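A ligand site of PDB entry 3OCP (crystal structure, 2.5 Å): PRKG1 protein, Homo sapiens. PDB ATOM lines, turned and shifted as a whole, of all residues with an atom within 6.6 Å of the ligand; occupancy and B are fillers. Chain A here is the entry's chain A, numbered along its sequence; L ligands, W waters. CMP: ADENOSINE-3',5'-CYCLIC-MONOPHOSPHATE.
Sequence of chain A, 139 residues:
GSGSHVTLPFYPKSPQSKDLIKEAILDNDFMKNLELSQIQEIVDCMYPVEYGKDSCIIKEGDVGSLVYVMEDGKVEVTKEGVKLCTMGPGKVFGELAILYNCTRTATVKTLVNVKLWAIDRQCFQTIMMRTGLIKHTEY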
ATOM      1  N   ASN A  28     -34.160 -17.565  21.299  1.00  0.00           N
ATOM      2  CA  ASN A  28     -33.352 -18.293  20.335  1.00  0.00           C
ATOM      3  C   ASN A  28     -33.293 -19.797  20.654  1.00  0.00           C
ATOM      4  O   ASN A  28     -32.802 -20.191  21.714  1.00  0.00           O
ATOM      5  CB  ASN A  28     -31.959 -17.692  20.217  1.00  0.00           C
ATOM      6  CG  ASN A  28     -31.096 -18.412  19.207  1.00  0.00           C
ATOM      7  OD1 ASN A  28     -30.364 -19.417  19.676  1.00  0.00           O
ATOM      8  ND2 ASN A  28     -31.115 -18.092  18.013  1.00  0.00           N
ATOM      9  N   PHE A  30     -31.378 -22.092  19.974  1.00  0.00           N
ATOM     10  CA  PHE A  30     -30.091 -22.708  20.257  1.00  0.00           C
ATOM     11  C   PHE A  30     -29.445 -22.180  21.531  1.00  0.00           C
ATOM     12  O   PHE A  30     -28.551 -22.825  22.079  1.00  0.00           O
ATOM     13  CB  PHE A  30     -29.152 -22.566  19.049  1.00  0.00           C
ATOM     14  CG  PHE A  30     -29.843 -22.778  17.725  1.00  0.00           C
ATOM     15  CD1 PHE A  30     -30.303 -24.027  17.369  1.00  0.00           C
ATOM     16  CD2 PHE A  30     -30.046 -21.729  16.860  1.00  0.00           C
ATOM     17  CE1 PHE A  30     -30.965 -24.225  16.161  1.00  0.00           C
ATOM     18  CE2 PHE A  30     -30.701 -21.917  15.636  1.00  0.00           C
ATOM     19  CZ  PHE A  30     -31.159 -23.164  15.293  1.00  0.00           C
ATOM     20  N   ILE A  58     -23.066  -9.516   7.672  1.00  0.00           N
ATOM     21  CA  ILE A  58     -22.524 -10.872   7.610  1.00  0.00           C
ATOM     22  C   ILE A  58     -22.613 -11.432   6.198  1.00  0.00           C
ATOM     23  O   ILE A  58     -23.686 -11.392   5.562  1.00  0.00           O
ATOM     24  CB  ILE A  58     -23.321 -11.832   8.522  1.00  0.00           C
ATOM     25  CG1 ILE A  58     -23.006 -11.554   9.988  1.00  0.00           C
ATOM     26  CG2 ILE A  58     -23.007 -13.282   8.175  1.00  0.00           C
ATOM     27  CD1 ILE A  58     -23.935 -12.278  10.917  1.00  0.00           C
ATOM     28  N   GLU A  60     -22.213 -14.838   3.802  1.00  0.00           N
ATOM     29  CA  GLU A  60     -22.184 -16.303   3.891  1.00  0.00           C
ATOM     30  C   GLU A  60     -20.827 -16.857   3.512  1.00  0.00           C
ATOM     31  O   GLU A  60     -20.162 -16.352   2.602  1.00  0.00           O
ATOM     32  CB  GLU A  60     -23.294 -16.956   3.042  1.00  0.00           C
ATOM     33  CG  GLU A  60     -23.307 -16.581   1.581  1.00  0.00           C
ATOM     34  CD  GLU A  60     -24.673 -16.782   0.928  1.00  0.00           C
ATOM     35  OE1 GLU A  60     -25.458 -15.803   0.846  1.00  0.00           O
ATOM     36  OE2 GLU A  60     -24.977 -17.911   0.517  1.00  0.00           O
ATOM     37  N   GLY A  64     -16.605 -16.394  11.270  1.00  0.00           N
ATOM     38  CA  GLY A  64     -17.382 -15.491  12.113  1.00  0.00           C
ATOM     39  C   GLY A  64     -16.745 -15.335  13.482  1.00  0.00           C
ATOM     40  O   GLY A  64     -16.077 -16.257  13.935  1.00  0.00           O
ATOM     41  N   LEU A  66     -18.489 -12.831  15.897  1.00  0.00           N
ATOM     42  CA  LEU A  66     -19.476 -12.126  16.719  1.00  0.00           C
ATOM     43  C   LEU A  66     -20.866 -12.692  16.579  1.00  0.00           C
ATOM     44  O   LEU A  66     -21.292 -13.067  15.474  1.00  0.00           O
ATOM     45  CB  LEU A  66     -19.522 -10.635  16.348  1.00  0.00           C
ATOM     46  CG  LEU A  66     -18.208  -9.860  16.500  1.00  0.00           C
ATOM     47  CD1 LEU A  66     -18.275  -8.490  15.839  1.00  0.00           C
ATOM     48  CD2 LEU A  66     -17.817  -9.727  17.953  1.00  0.00           C
ATOM     49  N   VAL A  77     -32.136 -11.868   5.741  1.00  0.00           N
ATOM     50  CA  VAL A  77     -31.221 -12.997   5.671  1.00  0.00           C
ATOM     51  C   VAL A  77     -31.403 -13.710   4.343  1.00  0.00           C
ATOM     52  O   VAL A  77     -32.508 -14.130   3.997  1.00  0.00           O
ATOM     53  CB  VAL A  77     -31.481 -14.001   6.803  1.00  0.00           C
ATOM     54  CG1 VAL A  77     -30.471 -15.124   6.762  1.00  0.00           C
ATOM     55  CG2 VAL A  77     -31.447 -13.298   8.140  1.00  0.00           C
ATOM     56  N   LYS A  79     -29.619 -16.706   1.590  1.00  0.00           N
ATOM     57  CA  LYS A  79     -28.600 -17.706   1.293  1.00  0.00           C
ATOM     58  C   LYS A  79     -28.572 -17.952  -0.215  1.00  0.00           C
ATOM     59  O   LYS A  79     -29.604 -18.249  -0.827  1.00  0.00           O
ATOM     60  CB  LYS A  79     -28.843 -19.004   2.043  1.00  0.00           C
ATOM     61  CG  LYS A  79     -27.719 -20.021   1.826  1.00  0.00           C
ATOM     62  CD  LYS A  79     -27.915 -21.296   2.630  1.00  0.00           C
ATOM     63  CE  LYS A  79     -26.775 -22.258   2.353  1.00  0.00           C
ATOM     64  NZ  LYS A  79     -25.446 -21.611   2.549  1.00  0.00           N
ATOM     65  N   LEU A  84     -34.340 -15.779   2.986  1.00  0.00           N
ATOM     66  CA  LEU A  84     -34.822 -16.748   3.966  1.00  0.00           C
ATOM     67  C   LEU A  84     -35.859 -16.114   4.898  1.00  0.00           C
ATOM     68  O   LEU A  84     -36.881 -16.726   5.214  1.00  0.00           O
ATOM     69  CB  LEU A  84     -33.662 -17.315   4.781  1.00  0.00           C
ATOM     70  CG  LEU A  84     -32.555 -17.998   3.981  1.00  0.00           C
ATOM     71  CD1 LEU A  84     -31.526 -18.639   4.898  1.00  0.00           C
ATOM     72  CD2 LEU A  84     -33.163 -19.029   3.049  1.00  0.00           C
ATOM     73  N   CYS A  85     -35.600 -14.881   5.324  1.00  0.00           N
ATOM     74  CA  CYS A  85     -36.497 -14.181   6.226  1.00  0.00           C
ATOM     75  C   CYS A  85     -36.068 -12.719   6.386  1.00  0.00           C
ATOM     76  O   CYS A  85     -35.186 -12.243   5.676  1.00  0.00           O
ATOM     77  CB  CYS A  85     -36.548 -14.903   7.569  1.00  0.00           C
ATOM     78  SG  CYS A  85     -34.979 -14.849   8.485  1.00  0.00           S
ATOM     79  N   MET A  87     -35.491 -10.023  10.060  1.00  0.00           N
ATOM     80  CA  MET A  87     -35.559  -9.969  11.521  1.00  0.00           C
ATOM     81  C   MET A  87     -35.644  -8.531  12.022  1.00  0.00           C
ATOM     82  O   MET A  87     -35.065  -7.623  11.431  1.00  0.00           O
ATOM     83  CB  MET A  87     -34.333 -10.652  12.153  1.00  0.00           C
ATOM     84  CG  MET A  87     -34.282 -12.152  11.954  1.00  0.00           C
ATOM     85  SD  MET A  87     -32.853 -12.957  12.730  1.00  0.00           S
ATOM     86  CE  MET A  87     -31.580 -12.588  11.536  1.00  0.00           C
ATOM     87  N   VAL A  92     -31.858 -12.639  17.940  1.00  0.00           N
ATOM     88  CA  VAL A  92     -30.440 -12.987  17.806  1.00  0.00           C
ATOM     89  C   VAL A  92     -30.116 -13.330  16.360  1.00  0.00           C
ATOM     90  O   VAL A  92     -30.950 -13.904  15.661  1.00  0.00           O
ATOM     91  CB  VAL A  92     -30.083 -14.198  18.691  1.00  0.00           C
ATOM     92  CG1 VAL A  92     -28.742 -14.803  18.279  1.00  0.00           C
ATOM     93  CG2 VAL A  92     -30.069 -13.802  20.166  1.00  0.00           C
ATOM     94  N   PHE A  93     -28.922 -12.974  15.886  1.00  0.00           N
ATOM     95  CA  PHE A  93     -28.406 -13.555  14.636  1.00  0.00           C
ATOM     96  C   PHE A  93     -26.878 -13.625  14.601  1.00  0.00           C
ATOM     97  O   PHE A  93     -26.197 -12.925  15.357  1.00  0.00           O
ATOM     98  CB  PHE A  93     -28.968 -12.853  13.381  1.00  0.00           C
ATOM     99  CG  PHE A  93     -28.438 -11.466  13.154  1.00  0.00           C
ATOM    100  CD1 PHE A  93     -29.171 -10.353  13.551  1.00  0.00           C
ATOM    101  CD2 PHE A  93     -27.214 -11.272  12.531  1.00  0.00           C
ATOM    102  CE1 PHE A  93     -28.679  -9.078  13.343  1.00  0.00           C
ATOM    103  CE2 PHE A  93     -26.716  -9.991  12.329  1.00  0.00           C
ATOM    104  CZ  PHE A  93     -27.448  -8.893  12.742  1.00  0.00           C
ATOM    105  N   GLY A  94     -26.345 -14.479  13.738  1.00  0.00           N
ATOM    106  CA  GLY A  94     -24.912 -14.683  13.677  1.00  0.00           C
ATOM    107  C   GLY A  94     -24.435 -15.534  14.842  1.00  0.00           C
ATOM    108  O   GLY A  94     -23.258 -15.521  15.174  1.00  0.00           O
ATOM    109  N   GLU A  95     -25.354 -16.275  15.441  1.00  0.00           N
ATOM    110  CA  GLU A  95     -25.003 -17.170  16.544  1.00  0.00           C
ATOM    111  C   GLU A  95     -24.436 -18.534  16.054  1.00  0.00           C
ATOM    112  O   GLU A  95     -23.613 -19.130  16.722  1.00  0.00           O
ATOM    113  CB  GLU A  95     -26.205 -17.386  17.477  1.00  0.00           C
ATOM    114  CG  GLU A  95     -27.213 -18.451  17.057  1.00  0.00           C
ATOM    115  CD  GLU A  95     -28.100 -18.019  15.901  1.00  0.00           C
ATOM    116  OE1 GLU A  95     -27.668 -17.155  15.108  1.00  0.00           O
ATOM    117  OE2 GLU A  95     -29.217 -18.548  15.780  1.00  0.00           O
ATOM    118  N   LEU A  96     -24.875 -19.001  14.906  1.00  0.00           N
ATOM    119  CA  LEU A  96     -24.487 -20.332  14.388  1.00  0.00           C
ATOM    120  C   LEU A  96     -22.961 -20.564  14.324  1.00  0.00           C
ATOM    121  O   LEU A  96     -22.444 -21.508  14.911  1.00  0.00           O
ATOM    122  CB  LEU A  96     -25.144 -20.596  13.037  1.00  0.00           C
ATOM    123  CG  LEU A  96     -26.504 -21.340  13.017  1.00  0.00           C
ATOM    124  CD1 LEU A  96     -27.233 -21.306  14.342  1.00  0.00           C
ATOM    125  CD2 LEU A  96     -27.393 -20.849  11.905  1.00  0.00           C
ATOM    126  N   ALA A  97     -22.255 -19.667  13.644  1.00  0.00           N
ATOM    127  CA  ALA A  97     -20.797 -19.757  13.535  1.00  0.00           C
ATOM    128  C   ALA A  97     -20.117 -19.819  14.897  1.00  0.00           C
ATOM    129  O   ALA A  97     -19.114 -20.497  15.072  1.00  0.00           O
ATOM    130  CB  ALA A  97     -20.259 -18.584  12.735  1.00  0.00           C
ATOM    131  N   ILE A  98     -20.665 -19.084  15.857  1.00  0.00           N
ATOM    132  CA  ILE A  98     -20.012 -18.951  17.146  1.00  0.00           C
ATOM    133  C   ILE A  98     -20.343 -20.158  18.020  1.00  0.00           C
ATOM    134  O   ILE A  98     -19.489 -20.654  18.742  1.00  0.00           O
ATOM    135  CB  ILE A  98     -20.420 -17.626  17.870  1.00  0.00           C
ATOM    136  CG1 ILE A  98     -19.593 -16.443  17.357  1.00  0.00           C
ATOM    137  CG2 ILE A  98     -20.199 -17.742  19.374  1.00  0.00           C
ATOM    138  CD1 ILE A  98     -19.573 -16.249  15.857  1.00  0.00           C
ATOM    139  N   CYS A 102     -18.665 -23.073  12.704  1.00  0.00           N
ATOM    140  CA  CYS A 102     -18.726 -23.191  11.243  1.00  0.00           C
ATOM    141  C   CYS A 102     -18.612 -21.806  10.624  1.00  0.00           C
ATOM    142  O   CYS A 102     -18.654 -20.807  11.335  1.00  0.00           O
ATOM    143  CB  CYS A 102     -20.041 -23.823  10.820  1.00  0.00           C
ATOM    144  SG  CYS A 102     -21.511 -22.996  11.532  1.00  0.00           S
ATOM    145  N   THR A 103     -18.466 -21.737   9.309  1.00  0.00           N
ATOM    146  CA  THR A 103     -18.492 -20.475   8.605  1.00  0.00           C
ATOM    147  C   THR A 103     -19.935 -19.989   8.587  1.00  0.00           C
ATOM    148  O   THR A 103     -20.854 -20.772   8.802  1.00  0.00           O
ATOM    149  CB  THR A 103     -18.024 -20.620   7.154  1.00  0.00           C
ATOM    150  OG1 THR A 103     -18.845 -21.598   6.492  1.00  0.00           O
ATOM    151  CG2 THR A 103     -16.570 -21.039   7.104  1.00  0.00           C
ATOM    152  N   ARG A 104     -20.119 -18.708   8.302  1.00  0.00           N
ATOM    153  CA  ARG A 104     -21.475 -18.162   8.291  1.00  0.00           C
ATOM    154  C   ARG A 104     -22.348 -18.946   7.330  1.00  0.00           C
ATOM    155  O   ARG A 104     -21.985 -19.161   6.186  1.00  0.00           O
ATOM    156  CB  ARG A 104     -21.430 -16.683   7.902  1.00  0.00           C
ATOM    157  CG  ARG A 104     -20.590 -15.844   8.832  1.00  0.00           C
ATOM    158  CD  ARG A 104     -21.285 -15.639  10.180  1.00  0.00           C
ATOM    159  NE  ARG A 104     -20.623 -14.594  10.936  1.00  0.00           N
ATOM    160  CZ  ARG A 104     -20.777 -14.399  12.247  1.00  0.00           C
ATOM    161  NH1 ARG A 104     -21.580 -15.191  12.935  1.00  0.00           N
ATOM    162  NH2 ARG A 104     -20.129 -13.411  12.847  1.00  0.00           N
ATOM    163  N   THR A 105     -23.517 -19.367   7.802  1.00  0.00           N
ATOM    164  CA  THR A 105     -24.431 -20.180   7.002  1.00  0.00           C
ATOM    165  C   THR A 105     -25.342 -19.357   6.087  1.00  0.00           C
ATOM    166  O   THR A 105     -26.131 -19.919   5.329  1.00  0.00           O
ATOM    167  CB  THR A 105     -25.326 -21.051   7.888  1.00  0.00           C
ATOM    168  OG1 THR A 105     -26.204 -20.224   8.662  1.00  0.00           O
ATOM    169  CG2 THR A 105     -24.463 -21.903   8.829  1.00  0.00           C
ATOM    170  N   ALA A 106     -25.258 -18.035   6.181  1.00  0.00           N
ATOM    171  CA  ALA A 106     -26.132 -17.160   5.405  1.00  0.00           C
ATOM    172  C   ALA A 106     -25.577 -15.753   5.379  1.00  0.00           C
ATOM    173  O   ALA A 106     -24.612 -15.448   6.065  1.00  0.00           O
ATOM    174  CB  ALA A 106     -27.546 -17.172   5.982  1.00  0.00           C
ATOM    175  N   THR A 107     -26.194 -14.905   4.568  1.00  0.00           N
ATOM    176  CA  THR A 107     -25.801 -13.506   4.475  1.00  0.00           C
ATOM    177  C   THR A 107     -26.866 -12.650   5.144  1.00  0.00           C
ATOM    178  O   THR A 107     -28.053 -12.913   5.020  1.00  0.00           O
ATOM    179  CB  THR A 107     -25.635 -13.067   3.021  1.00  0.00           C
ATOM    180  OG1 THR A 107     -24.419 -13.629   2.499  1.00  0.00           O
ATOM    181  CG2 THR A 107     -25.581 -11.561   2.915  1.00  0.00           C
ATOM    182  N   VAL A 108     -26.418 -11.630   5.864  1.00  0.00           N
ATOM    183  CA  VAL A 108     -27.338 -10.722   6.569  1.00  0.00           C
ATOM    184  C   VAL A 108     -27.038  -9.263   6.208  1.00  0.00           C
ATOM    185  O   VAL A 108     -25.910  -8.789   6.400  1.00  0.00           O
ATOM    186  CB  VAL A 108     -27.255 -10.934   8.100  1.00  0.00           C
ATOM    187  CG1 VAL A 108     -28.194  -9.987   8.831  1.00  0.00           C
ATOM    188  CG2 VAL A 108     -27.586 -12.383   8.442  1.00  0.00           C
HETATM  189  P   CMP L   1     -24.579 -17.508  11.165  1.00  0.00           P
HETATM  190  O1P CMP L   1     -24.441 -18.699  10.314  1.00  0.00           O
HETATM  191  O2P CMP L   1     -23.426 -17.332  12.323  1.00  0.00           O
HETATM  192  O5' CMP L   1     -24.494 -16.194  10.315  1.00  0.00           O
HETATM  193  C5' CMP L   1     -25.628 -16.059   9.467  1.00  0.00           C
HETATM  194  C4' CMP L   1     -26.853 -16.122  10.318  1.00  0.00           C
HETATM  195  O4' CMP L   1     -28.089 -16.072   9.576  1.00  0.00           O
HETATM  196  C3' CMP L   1     -26.997 -17.409  11.087  1.00  0.00           C
HETATM  197  O3' CMP L   1     -25.959 -17.543  12.043  1.00  0.00           O
HETATM  198  C2' CMP L   1     -28.403 -17.232  11.638  1.00  0.00           C
HETATM  199  O2' CMP L   1     -28.412 -16.295  12.713  1.00  0.00           O
HETATM  200  C1' CMP L   1     -29.106 -16.613  10.415  1.00  0.00           C
HETATM  201  N9  CMP L   1     -29.812 -17.647   9.635  1.00  0.00           N
HETATM  202  C8  CMP L   1     -29.250 -18.567   8.856  1.00  0.00           C
HETATM  203  N7  CMP L   1     -30.245 -19.319   8.299  1.00  0.00           N
HETATM  204  C5  CMP L   1     -31.445 -18.830   8.763  1.00  0.00           C
HETATM  205  C6  CMP L   1     -32.829 -19.221   8.505  1.00  0.00           C
HETATM  206  N6  CMP L   1     -33.101 -20.330   7.611  1.00  0.00           N
HETATM  207  N1  CMP L   1     -33.814 -18.580   9.075  1.00  0.00           N
HETATM  208  C2  CMP L   1     -33.547 -17.523   9.926  1.00  0.00           C
HETATM  209  N3  CMP L   1     -32.208 -17.139  10.163  1.00  0.00           N
HETATM  210  C4  CMP L   1     -31.199 -17.812   9.572  1.00  0.00           C
HETATM  211  O   HOH W   1     -36.838 -18.970   8.735  1.00  0.00           O
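An oxygen (O2P) of the ligand is in salt-bridge range of the guanidinium group (NH1) of Arg 104 (2.9 Å).
The backbone NH of Gly 94 is in hydrogen-bond range of an oxygen (O2') of the ligand (2.9 Å).
N of Leu 96 sits close to O3' of the ligand, 3.4 Å away.
O1P of the ligand sits at hydrogen-bond distance from OG1 of Thr 105 (2.9 Å).
N of Thr 105 is in hydrogen-bond range of O1P of the ligand.
N of Ala 97 is in hydrogen-bond range of O2P of the ligand (2.9 Å).
An oxygen (O2') of the ligand lies within hydrogen-bond range of the side-chain carboxylate (OE1) of Glu 95 (2.7 Å).
The backbone NH of Val 108 is in hydrogen-bond range of the backbone carbonyl oxygen of Ile 58 (2.8 Å).
The side-chain carboxylate (OE2) of Glu 95 lies within hydrogen-bond range of the side-chain amide nitrogen (ND2) of Asn 28 (3.0 Å).
The guanidinium group (NH1) of Arg 104 sits at hydrogen-bond distance from the backbone carbonyl oxygen (O) of Gly 94.
N of Leu 84 sits at hydrogen-bond distance from O of Val 77 (2.7 Å).
The backbone NH (N) of Glu 60 lies within hydrogen-bond range of the backbone carbonyl oxygen (O) of Ala 106 (3.4 Å).
The guanidinium group of Arg 104 sits at hydrogen-bond distance from the backbone carbonyl oxygen of Leu 66 (2.9 Å).
The backbone NH of Val 77 sits at hydrogen-bond distance from the backbone carbonyl oxygen of Cys 85, at 3.1 Å.
The backbone carbonyl oxygen (O) of Thr 105 lies within hydrogen-bond range of the side-chain amino group (NZ) of Lys 79.
CG2 of Ile 58 touches O5' of the ligand, at 3.9 Å.
Val 77 touches the ligand (CG1 to O4', 3.8 Å).
Leu 84 touches the ligand (CD1 to N6, 3.6 Å).
Cys 85 touches the ligand (SG to C2, 3.4 Å).
CA of Phe 93 touches O2' of the ligand (3.3 Å).
O of Ala 106 touches C5' of the ligand (3.6 Å).
CG2 of Val 108 touches O4' of the ligand, 3.9 Å away.
Hydrophobic or aromatic side chains within 4 Å of the ligand: Ile 58, Val 77, Leu 84, Phe 93, Leu 96, Ala 97, Ala 106 and Val 108.
Of the 25 residues printed, 13 come within 4 Å of the ligand.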
